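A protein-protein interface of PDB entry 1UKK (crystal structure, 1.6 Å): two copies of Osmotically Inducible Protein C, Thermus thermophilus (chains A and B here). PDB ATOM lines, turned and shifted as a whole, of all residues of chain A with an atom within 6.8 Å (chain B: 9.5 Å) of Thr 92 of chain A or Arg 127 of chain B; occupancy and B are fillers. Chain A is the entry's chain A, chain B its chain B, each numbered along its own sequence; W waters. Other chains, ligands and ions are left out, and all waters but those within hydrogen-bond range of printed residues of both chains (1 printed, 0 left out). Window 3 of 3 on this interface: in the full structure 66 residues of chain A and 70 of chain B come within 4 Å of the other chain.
O of Pro 2 of chain B is in hydrogen-bond range of N of Leu 84 of chain A, 3.0 Å away.
O of Pro 91 of chain A is in hydrogen-bond range of NH2 of Arg 127 of chain B.
OG1 of Thr 92 of chain A lies within hydrogen-bond range of NH2 of Arg 127 of chain B (2.9 Å).
The backbone NH (N) of Gly 131 of chain B sits at hydrogen-bond distance from the backbone carbonyl oxygen (O) of Ala 128 of chain A (2.9 Å).
The backbone carbonyl oxygen (O) of Ala 128 of chain B sits at hydrogen-bond distance from the backbone NH (N) of Gly 131 of chain A (3.1 Å).
The backbone carbonyl oxygen (O) of Ala 128 of chain A sits close to the backbone carbonyl oxygen (O) of Ala 128 of chain B.
The backbone NH (N) of Thr 94 of chain A is in hydrogen-bond range of the backbone carbonyl oxygen (O) of His 83 of chain A (3.0 Å).
The backbone carbonyl oxygen of Arg 95 of chain A lies within hydrogen-bond range of the backbone NH of His 83 of chain A (2.9 Å).
N of Thr 92 of chain A lies within hydrogen-bond range of O of Glu 85 of chain A (2.7 Å).
OG1 of Thr 92 of chain A lies within hydrogen-bond range of O of Val 87 of chain A.
Among the printed residues, pairs that only touch across the chains: Leu 129 of chain A with Ala 128 of chain B, Ala 128 of chain A with Leu 129 of chain B, Pro 91 of chain A with Pro 124 of chain B, Ala 130 of chain A with Ala 128 of chain B, Gly 131 of chain A with Arg 127 of chain B, Leu 129 of chain A with Leu 129 of chain B, Ala 130 of chain A with Gly 131 of chain B, His 83 of chain A with Pro 2 of chain B, Ala 128 of chain A with Ala 130 of chain B, His 83 of chain A with Val 3 of chain B and Ala 128 of chain A with Val 132 of chain B.
Of chain B, only Arg 127 (2.9 Å) comes within 4 Å of Thr 92 of chain A.
No residue of chain B comes within 4 Å of Lys 90 of chain A.
Pro 91 of chain A touches just these residues of chain B: Pro 124 and Arg 127.
Of the printed residues of chain A, Leu 129 of chain B touches Ala 128 and Leu 129.
Of the printed residues of chain A, Pro 124 of chain B touches Pro 91.
Printed residues of chain A within 4 Å of Ala 128 of chain B: Ala 128, Leu 129, Ala 130 and Gly 131.
Of the printed residues of chain A, Val 3 of chain B touches His 83.
Of the printed residues of chain B, His 83 of chain A touches Pro 2 (3.7 Å) and Val 3 (3.8 Å).
The nearest residue of chain B that does not touch Thr 92 of chain A is Pro 124 of chain B (4.4 Å).
Of the 22 printed residues of chain B, 9 touch a printed residue of chain A.
Hydrophobic or aromatic side chains of chain B that line the printed part of chain A: Pro 2, Val 3, Pro 124, Leu 129 and Val 132.
Printed residues of chain A that touch a printed residue of chain B: His 83, Leu 84, Pro 91, Thr 92, Ala 128, Leu 129, Ala 130 and Gly 131.
Among the printed residues, 17 pairs touch across the chains.
Among the printed residues, no Asp or Glu carboxylate lies within 4 Å of a Lys or Arg side-chain nitrogen of the other chain.
Ala 128 of chain B touches its own counterpart, Ala 128 of chain A.
Ala 128 of chain A touches Ala 130 of chain B, and with the chains exchanged Ala 130 of chain A touches Ala 128 of chain B.
Ala 128 of chain A touches Gly 131 of chain B, and with the chains exchanged Gly 131 of chain A touches Ala 128 of chain B.
Ala 128 of chain A touches Val 132 of chain B, but with the chains exchanged Val 132 of chain A does not touch Ala 128 of chain B (4.1 Å).
Of the 17 pairs that touch across the chains among the printed residues, 8 have their exchanged pair printed and touching as well.
Water W1 lies within hydrogen-bond range of the backbone carbonyl oxygen of Pro 124 of chain B and the backbone NH of Leu 93 of chain A.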
ATOM      1  N   GLU A  47      23.307 -33.003  31.787  1.00  0.00           N
ATOM      2  CA  GLU A  47      22.572 -33.339  30.584  1.00  0.00           C
ATOM      3  C   GLU A  47      21.249 -34.088  30.879  1.00  0.00           C
ATOM      4  O   GLU A  47      20.242 -33.780  30.232  1.00  0.00           O
ATOM      5  CB  GLU A  47      23.455 -34.146  29.631  1.00  0.00           C
ATOM      6  CG  GLU A  47      24.592 -33.373  28.908  1.00  0.00           C
ATOM      7  CD  GLU A  47      25.698 -32.832  29.845  1.00  0.00           C
ATOM      8  OE1 GLU A  47      26.083 -33.565  30.831  1.00  0.00           O
ATOM      9  OE2 GLU A  47      26.080 -31.678  29.680  1.00  0.00           O
ATOM     10  N   HIS A  83      22.060 -35.408  23.458  1.00  0.00           N
ATOM     11  CA  HIS A  83      23.306 -35.934  22.897  1.00  0.00           C
ATOM     12  C   HIS A  83      24.433 -35.009  23.268  1.00  0.00           C
ATOM     13  O   HIS A  83      24.384 -33.816  22.972  1.00  0.00           O
ATOM     14  CB  HIS A  83      23.175 -36.034  21.356  1.00  0.00           C
ATOM     15  CG  HIS A  83      22.204 -37.089  20.915  1.00  0.00           C
ATOM     16  ND1 HIS A  83      22.537 -38.098  20.038  1.00  0.00           N
ATOM     17  CD2 HIS A  83      20.906 -37.299  21.249  1.00  0.00           C
ATOM     18  CE1 HIS A  83      21.501 -38.903  19.869  1.00  0.00           C
ATOM     19  NE2 HIS A  83      20.497 -38.448  20.600  1.00  0.00           N
ATOM     20  N   LEU A  84      25.452 -35.557  23.931  1.00  0.00           N
ATOM     21  CA  LEU A  84      26.635 -34.818  24.325  1.00  0.00           C
ATOM     22  C   LEU A  84      27.802 -35.403  23.546  1.00  0.00           C
ATOM     23  O   LEU A  84      28.075 -36.582  23.670  1.00  0.00           O
ATOM     24  CB  LEU A  84      26.882 -35.004  25.846  1.00  0.00           C
ATOM     25  CG  LEU A  84      28.148 -34.332  26.407  1.00  0.00           C
ATOM     26  CD1 LEU A  84      28.041 -32.837  26.279  1.00  0.00           C
ATOM     27  CD2 LEU A  84      28.456 -34.751  27.884  1.00  0.00           C
ATOM     28  N   GLU A  85      28.445 -34.582  22.737  1.00  0.00           N
ATOM     29  CA  GLU A  85      29.591 -35.008  21.929  1.00  0.00           C
ATOM     30  C   GLU A  85      30.829 -34.233  22.343  1.00  0.00           C
ATOM     31  O   GLU A  85      30.747 -33.248  23.086  1.00  0.00           O
ATOM     32  CB  GLU A  85      29.318 -34.782  20.437  1.00  0.00           C
ATOM     33  CG  GLU A  85      28.156 -35.565  19.832  1.00  0.00           C
ATOM     34  CD  GLU A  85      27.835 -36.888  20.519  1.00  0.00           C
ATOM     35  OE1 GLU A  85      28.773 -37.652  20.864  1.00  0.00           O
ATOM     36  OE2 GLU A  85      26.626 -37.180  20.702  1.00  0.00           O
ATOM     37  N   VAL A  86      31.983 -34.688  21.866  1.00  0.00           N
ATOM     38  CA  VAL A  86      33.268 -34.197  22.379  1.00  0.00           C
ATOM     39  C   VAL A  86      33.884 -33.278  21.322  1.00  0.00           C
ATOM     40  O   VAL A  86      35.109 -33.098  21.248  1.00  0.00           O
ATOM     41  CB  VAL A  86      34.189 -35.385  22.768  1.00  0.00           C
ATOM     42  CG1 VAL A  86      35.203 -34.968  23.836  1.00  0.00           C
ATOM     43  CG2 VAL A  86      33.347 -36.562  23.291  1.00  0.00           C
ATOM     44  N   VAL A  87      32.978 -32.650  20.561  1.00  0.00           N
ATOM     45  CA  VAL A  87      33.252 -32.011  19.291  1.00  0.00           C
ATOM     46  C   VAL A  87      32.902 -30.511  19.382  1.00  0.00           C
ATOM     47  O   VAL A  87      31.856 -30.151  19.937  1.00  0.00           O
ATOM     48  CB  VAL A  87      32.408 -32.728  18.220  1.00  0.00           C
ATOM     49  CG1 VAL A  87      32.713 -32.249  16.799  1.00  0.00           C
ATOM     50  CG2 VAL A  87      32.613 -34.250  18.349  1.00  0.00           C
ATOM     51  N   ASP A  88      33.756 -29.629  18.851  1.00  0.00           N
ATOM     52  CA  ASP A  88      34.940 -30.012  18.069  1.00  0.00           C
ATOM     53  C   ASP A  88      36.239 -29.714  18.840  1.00  0.00           C
ATOM     54  O   ASP A  88      36.748 -28.590  18.830  1.00  0.00           O
ATOM     55  CB  ASP A  88      34.923 -29.311  16.703  1.00  0.00           C
ATOM     56  CG  ASP A  88      35.547 -30.164  15.596  1.00  0.00           C
ATOM     57  OD1 ASP A  88      35.380 -31.407  15.631  1.00  0.00           O
ATOM     58  OD2 ASP A  88      36.212 -29.679  14.644  1.00  0.00           O
ATOM     59  N   GLY A  89      36.767 -30.740  19.509  1.00  0.00           N
ATOM     60  CA  GLY A  89      37.674 -30.532  20.621  1.00  0.00           C
ATOM     61  C   GLY A  89      36.995 -29.937  21.862  1.00  0.00           C
ATOM     62  O   GLY A  89      37.676 -29.658  22.851  1.00  0.00           O
ATOM     63  N   LYS A  90      35.670 -29.738  21.828  1.00  0.00           N
ATOM     64  CA  LYS A  90      34.935 -29.316  23.029  1.00  0.00           C
ATOM     65  C   LYS A  90      33.580 -30.043  23.144  1.00  0.00           C
ATOM     66  O   LYS A  90      32.886 -30.200  22.142  1.00  0.00           O
ATOM     67  CB  LYS A  90      34.740 -27.794  23.064  1.00  0.00           C
ATOM     68  CG  LYS A  90      34.226 -27.129  21.774  1.00  0.00           C
ATOM     69  CD  LYS A  90      34.649 -25.647  21.725  1.00  0.00           C
ATOM     70  CE  LYS A  90      33.642 -24.780  21.004  1.00  0.00           C
ATOM     71  NZ  LYS A  90      34.104 -23.354  20.926  1.00  0.00           N
ATOM     72  N   PRO A  91      33.207 -30.477  24.357  1.00  0.00           N
ATOM     73  CA  PRO A  91      31.936 -31.197  24.553  1.00  0.00           C
ATOM     74  C   PRO A  91      30.754 -30.299  24.303  1.00  0.00           C
ATOM     75  O   PRO A  91      30.722 -29.165  24.778  1.00  0.00           O
ATOM     76  CB  PRO A  91      31.997 -31.637  26.022  1.00  0.00           C
ATOM     77  CG  PRO A  91      32.913 -30.592  26.684  1.00  0.00           C
ATOM     78  CD  PRO A  91      33.946 -30.315  25.625  1.00  0.00           C
ATOM     79  N   THR A  92      29.793 -30.780  23.532  1.00  0.00           N
ATOM     80  CA  THR A  92      28.696 -29.930  23.101  1.00  0.00           C
ATOM     81  C   THR A  92      27.380 -30.681  23.146  1.00  0.00           C
ATOM     82  O   THR A  92      27.369 -31.854  22.881  1.00  0.00           O
ATOM     83  CB  THR A  92      28.965 -29.475  21.673  1.00  0.00           C
ATOM     84  OG1 THR A  92      30.312 -28.969  21.585  1.00  0.00           O
ATOM     85  CG2 THR A  92      28.052 -28.278  21.307  1.00  0.00           C
ATOM     86  N   LEU A  93      26.286 -29.991  23.492  1.00  0.00           N
ATOM     87  CA  LEU A  93      24.940 -30.568  23.376  1.00  0.00           C
ATOM     88  C   LEU A  93      24.523 -30.355  21.951  1.00  0.00           C
ATOM     89  O   LEU A  93      24.214 -29.238  21.538  1.00  0.00           O
ATOM     90  CB  LEU A  93      23.940 -29.925  24.342  1.00  0.00           C
ATOM     91  CG  LEU A  93      24.280 -29.992  25.825  1.00  0.00           C
ATOM     92  CD1 LEU A  93      22.992 -29.932  26.697  1.00  0.00           C
ATOM     93  CD2 LEU A  93      25.091 -31.197  26.148  1.00  0.00           C
ATOM     94  N   THR A  94      24.563 -31.434  21.197  1.00  0.00           N
ATOM     95  CA  THR A  94      24.413 -31.347  19.735  1.00  0.00           C
ATOM     96  C   THR A  94      23.026 -31.563  19.199  1.00  0.00           C
ATOM     97  O   THR A  94      22.666 -30.995  18.161  1.00  0.00           O
ATOM     98  CB  THR A  94      25.349 -32.328  19.042  1.00  0.00           C
ATOM     99  OG1 THR A  94      25.144 -33.660  19.516  1.00  0.00           O
ATOM    100  CG2 THR A  94      26.826 -31.994  19.366  1.00  0.00           C
ATOM    101  N   ARG A  95      22.268 -32.410  19.883  1.00  0.00           N
ATOM    102  CA  ARG A  95      20.977 -32.864  19.385  1.00  0.00           C
ATOM    103  C   ARG A  95      20.114 -33.198  20.581  1.00  0.00           C
ATOM    104  O   ARG A  95      20.612 -33.714  21.562  1.00  0.00           O
ATOM    105  CB  ARG A  95      21.207 -34.097  18.520  1.00  0.00           C
ATOM    106  CG  ARG A  95      20.008 -34.750  17.902  1.00  0.00           C
ATOM    107  CD  ARG A  95      20.429 -35.937  17.008  1.00  0.00           C
ATOM    108  NE  ARG A  95      19.483 -37.054  17.117  1.00  0.00           N
ATOM    109  CZ  ARG A  95      19.794 -38.357  17.075  1.00  0.00           C
ATOM    110  NH1 ARG A  95      21.050 -38.776  16.937  1.00  0.00           N
ATOM    111  NH2 ARG A  95      18.820 -39.257  17.182  1.00  0.00           N
ATOM    112  N   ALA A 128      15.206 -21.203  25.043  1.00  0.00           N
ATOM    113  CA  ALA A 128      16.437 -21.016  25.807  1.00  0.00           C
ATOM    114  C   ALA A 128      17.569 -21.894  25.255  1.00  0.00           C
ATOM    115  O   ALA A 128      18.713 -21.456  25.145  1.00  0.00           O
ATOM    116  CB  ALA A 128      16.201 -21.342  27.309  1.00  0.00           C
ATOM    117  N   LEU A 129      17.230 -23.121  24.884  1.00  0.00           N
ATOM    118  CA  LEU A 129      18.209 -24.069  24.345  1.00  0.00           C
ATOM    119  C   LEU A 129      18.489 -23.832  22.859  1.00  0.00           C
ATOM    120  O   LEU A 129      18.658 -24.800  22.118  1.00  0.00           O
ATOM    121  CB  LEU A 129      17.727 -25.518  24.562  1.00  0.00           C
ATOM    122  CG  LEU A 129      17.773 -26.007  26.017  1.00  0.00           C
ATOM    123  CD1 LEU A 129      16.949 -27.279  26.218  1.00  0.00           C
ATOM    124  CD2 LEU A 129      19.228 -26.211  26.455  1.00  0.00           C
ATOM    125  N   ALA A 130      18.590 -22.562  22.443  1.00  0.00           N
ATOM    126  CA  ALA A 130      18.833 -22.181  21.047  1.00  0.00           C
ATOM    127  C   ALA A 130      20.175 -22.673  20.493  1.00  0.00           C
ATOM    128  O   ALA A 130      20.307 -22.888  19.287  1.00  0.00           O
ATOM    129  CB  ALA A 130      18.727 -20.638  20.897  1.00  0.00           C
ATOM    130  N   GLY A 131      21.153 -22.878  21.377  1.00  0.00           N
ATOM    131  CA  GLY A 131      22.477 -23.350  21.014  1.00  0.00           C
ATOM    132  C   GLY A 131      22.553 -24.803  20.568  1.00  0.00           C
ATOM    133  O   GLY A 131      23.558 -25.226  20.002  1.00  0.00           O
ATOM    134  N   VAL A 132      21.502 -25.578  20.830  1.00  0.00           N
ATOM    135  CA  VAL A 132      21.383 -26.930  20.291  1.00  0.00           C
ATOM    136  C   VAL A 132      21.022 -26.862  18.790  1.00  0.00           C
ATOM    137  O   VAL A 132      20.017 -26.267  18.406  1.00  0.00           O
ATOM    138  CB  VAL A 132      20.353 -27.742  21.093  1.00  0.00           C
ATOM    139  CG1 VAL A 132      20.187 -29.121  20.519  1.00  0.00           C
ATOM    140  CG2 VAL A 132      20.769 -27.823  22.597  1.00  0.00           C
ATOM    141  N   LYS A 133      21.862 -27.489  17.963  1.00  0.00           N
ATOM    142  CA  LYS A 133      21.761 -27.476  16.494  1.00  0.00           C
ATOM    143  C   LYS A 133      20.542 -28.220  15.926  1.00  0.00           C
ATOM    144  O   LYS A 133      20.012 -27.885  14.860  1.00  0.00           O
ATOM    145  CB  LYS A 133      23.038 -28.108  15.889  1.00  0.00           C
ATOM    146  CG  LYS A 133      24.197 -27.141  15.720  1.00  0.00           C
ATOM    147  CD  LYS A 133      25.426 -27.801  15.033  1.00  0.00           C
ATOM    148  CE  LYS A 133      26.662 -26.837  15.009  1.00  0.00           C
ATOM    149  NZ  LYS A 133      27.515 -26.887  13.740  1.00  0.00           N
ATOM    150  N   PRO B   2      27.993 -39.338  24.888  1.00  0.00           N
ATOM    151  CA  PRO B   2      26.857 -40.107  25.477  1.00  0.00           C
ATOM    152  C   PRO B   2      25.486 -39.561  25.072  1.00  0.00           C
ATOM    153  O   PRO B   2      25.379 -38.489  24.509  1.00  0.00           O
ATOM    154  CB  PRO B   2      27.055 -39.964  26.993  1.00  0.00           C
ATOM    155  CG  PRO B   2      28.212 -39.093  27.221  1.00  0.00           C
ATOM    156  CD  PRO B   2      28.916 -38.806  25.906  1.00  0.00           C
ATOM    157  N   VAL B   3      24.452 -40.333  25.352  1.00  0.00           N
ATOM    158  CA  VAL B   3      23.066 -39.889  25.184  1.00  0.00           C
ATOM    159  C   VAL B   3      22.424 -40.018  26.551  1.00  0.00           C
ATOM    160  O   VAL B   3      22.354 -41.107  27.142  1.00  0.00           O
ATOM    161  CB  VAL B   3      22.311 -40.795  24.171  1.00  0.00           C
ATOM    162  CG1 VAL B   3      20.794 -40.340  24.053  1.00  0.00           C
ATOM    163  CG2 VAL B   3      23.057 -40.741  22.832  1.00  0.00           C
ATOM    164  N   HIS B  54      22.784 -26.041  35.231  1.00  0.00           N
ATOM    165  CA  HIS B  54      23.723 -24.997  34.989  1.00  0.00           C
ATOM    166  C   HIS B  54      24.709 -24.802  36.139  1.00  0.00           C
ATOM    167  O   HIS B  54      25.943 -24.596  35.893  1.00  0.00           O
ATOM    168  CB  HIS B  54      22.945 -23.739  34.746  1.00  0.00           C
ATOM    169  CG  HIS B  54      23.704 -22.740  33.955  1.00  0.00           C
ATOM    170  ND1 HIS B  54      23.212 -21.482  33.705  1.00  0.00           N
ATOM    171  CD2 HIS B  54      24.916 -22.797  33.351  1.00  0.00           C
ATOM    172  CE1 HIS B  54      24.102 -20.795  33.007  1.00  0.00           C
ATOM    173  NE2 HIS B  54      25.138 -21.571  32.764  1.00  0.00           N
ATOM    174  N   CSD B  57      27.179 -27.741  35.759  1.00  0.00           N
ATOM    175  CA  CSD B  57      28.133 -27.421  34.715  1.00  0.00           C
ATOM    176  CB  CSD B  57      27.295 -26.911  33.535  1.00  0.00           C
ATOM    177  SG  CSD B  57      28.451 -26.497  32.143  1.00  0.00           S
ATOM    178  C   CSD B  57      29.157 -26.419  35.213  1.00  0.00           C
ATOM    179  O   CSD B  57      30.361 -26.677  35.169  1.00  0.00           O
ATOM    180  OD1 CSD B  57      28.786 -28.072  31.595  1.00  0.00           O
ATOM    181  OD2 CSD B  57      27.498 -25.826  31.101  1.00  0.00           O
ATOM    182  N   ALA B  61      33.193 -26.817  35.471  1.00  0.00           N
ATOM    183  CA  ALA B  61      33.969 -26.126  34.468  1.00  0.00           C
ATOM    184  C   ALA B  61      34.979 -25.180  35.152  1.00  0.00           C
ATOM    185  O   ALA B  61      36.147 -25.056  34.703  1.00  0.00           O
ATOM    186  CB  ALA B  61      33.063 -25.329  33.470  1.00  0.00           C
ATOM    187  N   ILE B  96      19.760 -15.656  33.780  1.00  0.00           N
ATOM    188  CA  ILE B  96      20.291 -16.578  34.798  1.00  0.00           C
ATOM    189  C   ILE B  96      21.388 -15.917  35.597  1.00  0.00           C
ATOM    190  O   ILE B  96      22.309 -15.330  35.014  1.00  0.00           O
ATOM    191  CB  ILE B  96      20.818 -17.881  34.112  1.00  0.00           C
ATOM    192  CG1 ILE B  96      19.648 -18.630  33.440  1.00  0.00           C
ATOM    193  CG2 ILE B  96      21.499 -18.808  35.115  1.00  0.00           C
ATOM    194  CD1 ILE B  96      20.004 -19.706  32.443  1.00  0.00           C
ATOM    195  N   ALA B 118      36.086 -16.063  32.664  1.00  0.00           N
ATOM    196  CA  ALA B 118      36.398 -16.810  31.433  1.00  0.00           C
ATOM    197  C   ALA B 118      35.742 -18.175  31.350  1.00  0.00           C
ATOM    198  O   ALA B 118      35.471 -18.676  30.253  1.00  0.00           O
ATOM    199  CB  ALA B 118      37.893 -16.957  31.290  1.00  0.00           C
ATOM    200  N   ALA B 119      35.469 -18.791  32.497  1.00  0.00           N
ATOM    201  CA  ALA B 119      34.882 -20.111  32.533  1.00  0.00           C
ATOM    202  C   ALA B 119      33.394 -20.075  32.218  1.00  0.00           C
ATOM    203  O   ALA B 119      32.829 -21.086  31.795  1.00  0.00           O
ATOM    204  CB  ALA B 119      35.107 -20.749  33.929  1.00  0.00           C
ATOM    205  N   LYS B 120      32.761 -18.927  32.422  1.00  0.00           N
ATOM    206  CA  LYS B 120      31.311 -18.855  32.384  1.00  0.00           C
ATOM    207  C   LYS B 120      30.758 -18.991  30.972  1.00  0.00           C
ATOM    208  O   LYS B 120      29.633 -19.472  30.796  1.00  0.00           O
ATOM    209  CB  LYS B 120      30.813 -17.577  33.058  1.00  0.00           C
ATOM    210  CG  LYS B 120      30.990 -16.306  32.276  1.00  0.00           C
ATOM    211  CD  LYS B 120      29.958 -15.252  32.694  1.00  0.00           C
ATOM    212  CE  LYS B 120      28.556 -15.607  32.209  1.00  0.00           C
ATOM    213  NZ  LYS B 120      27.883 -14.429  31.583  1.00  0.00           N
ATOM    214  N   GLU B 121      31.537 -18.560  29.982  1.00  0.00           N
ATOM    215  CA  GLU B 121      31.231 -18.880  28.579  1.00  0.00           C
ATOM    216  C   GLU B 121      31.461 -20.362  28.236  1.00  0.00           C
ATOM    217  O   GLU B 121      30.498 -21.136  28.188  1.00  0.00           O
ATOM    218  CB  GLU B 121      31.991 -17.985  27.581  1.00  0.00           C
ATOM    219  CG  GLU B 121      33.461 -17.713  27.881  1.00  0.00           C
ATOM    220  CD  GLU B 121      33.765 -16.227  28.082  1.00  0.00           C
ATOM    221  OE1 GLU B 121      32.900 -15.367  27.781  1.00  0.00           O
ATOM    222  OE2 GLU B 121      34.887 -15.909  28.540  1.00  0.00           O
ATOM    223  N   GLY B 122      32.720 -20.759  28.028  1.00  0.00           N
ATOM    224  CA  GLY B 122      33.047 -21.954  27.254  1.00  0.00           C
ATOM    225  C   GLY B 122      32.716 -23.348  27.777  1.00  0.00           C
ATOM    226  O   GLY B 122      33.637 -24.132  27.974  1.00  0.00           O
ATOM    227  N   CYS B 123      31.432 -23.682  27.952  1.00  0.00           N
ATOM    228  CA  CYS B 123      31.025 -25.054  28.316  1.00  0.00           C
ATOM    229  C   CYS B 123      29.576 -25.459  27.925  1.00  0.00           C
ATOM    230  O   CYS B 123      28.749 -24.603  27.625  1.00  0.00           O
ATOM    231  CB  CYS B 123      31.353 -25.336  29.784  1.00  0.00           C
ATOM    232  SG  CYS B 123      32.965 -26.181  29.871  1.00  0.00           S
ATOM    233  N   PRO B 124      29.306 -26.765  27.868  1.00  0.00           N
ATOM    234  CA  PRO B 124      28.176 -27.291  27.077  1.00  0.00           C
ATOM    235  C   PRO B 124      26.778 -26.734  27.412  1.00  0.00           C
ATOM    236  O   PRO B 124      26.043 -26.361  26.481  1.00  0.00           O
ATOM    237  CB  PRO B 124      28.232 -28.811  27.328  1.00  0.00           C
ATOM    238  CG  PRO B 124      29.618 -29.108  27.875  1.00  0.00           C
ATOM    239  CD  PRO B 124      30.091 -27.844  28.504  1.00  0.00           C
ATOM    240  N   VAL B 125      26.408 -26.727  28.695  1.00  0.00           N
ATOM    241  CA  VAL B 125      25.099 -26.188  29.117  1.00  0.00           C
ATOM    242  C   VAL B 125      24.985 -24.679  28.864  1.00  0.00           C
ATOM    243  O   VAL B 125      23.994 -24.226  28.298  1.00  0.00           O
ATOM    244  CB  VAL B 125      24.744 -26.536  30.608  1.00  0.00           C
ATOM    245  CG1 VAL B 125      23.445 -25.851  31.057  1.00  0.00           C
ATOM    246  CG2 VAL B 125      24.622 -28.029  30.760  1.00  0.00           C
ATOM    247  N   SER B 126      25.997 -23.914  29.264  1.00  0.00           N
ATOM    248  CA  SER B 126      26.012 -22.465  29.059  1.00  0.00           C
ATOM    249  C   SER B 126      25.911 -22.094  27.575  1.00  0.00           C
ATOM    250  O   SER B 126      25.256 -21.126  27.243  1.00  0.00           O
ATOM    251  CB  SER B 126      27.270 -21.852  29.667  1.00  0.00           C
ATOM    252  OG  SER B 126      27.288 -22.043  31.085  1.00  0.00           O
ATOM    253  N   ARG B 127      26.533 -22.897  26.701  1.00  0.00           N
ATOM    254  CA  ARG B 127      26.535 -22.638  25.247  1.00  0.00           C
ATOM    255  C   ARG B 127      25.236 -23.123  24.616  1.00  0.00           C
ATOM    256  O   ARG B 127      24.736 -22.540  23.646  1.00  0.00           O
ATOM    257  CB  ARG B 127      27.744 -23.305  24.569  1.00  0.00           C
ATOM    258  CG  ARG B 127      29.047 -22.481  24.703  1.00  0.00           C
ATOM    259  CD  ARG B 127      30.350 -23.287  24.667  1.00  0.00           C
ATOM    260  NE  ARG B 127      30.144 -24.550  23.964  1.00  0.00           N
ATOM    261  CZ  ARG B 127      30.672 -25.725  24.284  1.00  0.00           C
ATOM    262  NH1 ARG B 127      31.505 -25.873  25.303  1.00  0.00           N
ATOM    263  NH2 ARG B 127      30.339 -26.777  23.559  1.00  0.00           N
ATOM    264  N   ALA B 128      24.685 -24.187  25.197  1.00  0.00           N
ATOM    265  CA  ALA B 128      23.412 -24.713  24.775  1.00  0.00           C
ATOM    266  C   ALA B 128      22.319 -23.715  25.123  1.00  0.00           C
ATOM    267  O   ALA B 128      21.332 -23.611  24.403  1.00  0.00           O
ATOM    268  CB  ALA B 128      23.148 -26.094  25.436  1.00  0.00           C
ATOM    269  N   LEU B 129      22.498 -22.966  26.214  1.00  0.00           N
ATOM    270  CA  LEU B 129      21.505 -21.974  26.647  1.00  0.00           C
ATOM    271  C   LEU B 129      21.799 -20.578  26.063  1.00  0.00           C
ATOM    272  O   LEU B 129      21.583 -19.555  26.727  1.00  0.00           O
ATOM    273  CB  LEU B 129      21.433 -21.910  28.184  1.00  0.00           C
ATOM    274  CG  LEU B 129      20.863 -23.139  28.915  1.00  0.00           C
ATOM    275  CD1 LEU B 129      21.084 -22.981  30.419  1.00  0.00           C
ATOM    276  CD2 LEU B 129      19.380 -23.366  28.600  1.00  0.00           C
ATOM    277  N   ALA B 130      22.275 -20.542  24.814  1.00  0.00           N
ATOM    278  CA  ALA B 130      22.503 -19.286  24.096  1.00  0.00           C
ATOM    279  C   ALA B 130      21.219 -18.507  23.931  1.00  0.00           C
ATOM    280  O   ALA B 130      21.235 -17.290  23.876  1.00  0.00           O
ATOM    281  CB  ALA B 130      23.130 -19.564  22.739  1.00  0.00           C
ATOM    282  N   GLY B 131      20.094 -19.212  23.890  1.00  0.00           N
ATOM    283  CA  GLY B 131      18.797 -18.573  23.933  1.00  0.00           C
ATOM    284  C   GLY B 131      18.520 -17.613  25.073  1.00  0.00           C
ATOM    285  O   GLY B 131      17.563 -16.862  24.999  1.00  0.00           O
ATOM    286  N   VAL B 132      19.298 -17.646  26.151  1.00  0.00           N
ATOM    287  CA  VAL B 132      18.992 -16.808  27.316  1.00  0.00           C
ATOM    288  C   VAL B 132      19.696 -15.457  27.207  1.00  0.00           C
ATOM    289  O   VAL B 132      20.930 -15.405  27.119  1.00  0.00           O
ATOM    290  CB  VAL B 132      19.395 -17.500  28.657  1.00  0.00           C
ATOM    291  CG1 VAL B 132      19.039 -16.592  29.829  1.00  0.00           C
ATOM    292  CG2 VAL B 132      18.700 -18.848  28.818  1.00  0.00           C
ATOM    293  N   VAL B 135      23.408 -13.909  31.159  1.00  0.00           N
ATOM    294  CA  VAL B 135      23.943 -14.747  32.237  1.00  0.00           C
ATOM    295  C   VAL B 135      24.971 -13.924  32.982  1.00  0.00           C
ATOM    296  O   VAL B 135      25.964 -13.469  32.409  1.00  0.00           O
ATOM    297  CB  VAL B 135      24.615 -16.029  31.697  1.00  0.00           C
ATOM    298  CG1 VAL B 135      24.955 -16.963  32.831  1.00  0.00           C
ATOM    299  CG2 VAL B 135      23.702 -16.719  30.695  1.00  0.00           C
HETATM  300  O   HOH W   1      26.723 -27.058  24.123  1.00  0.00           O
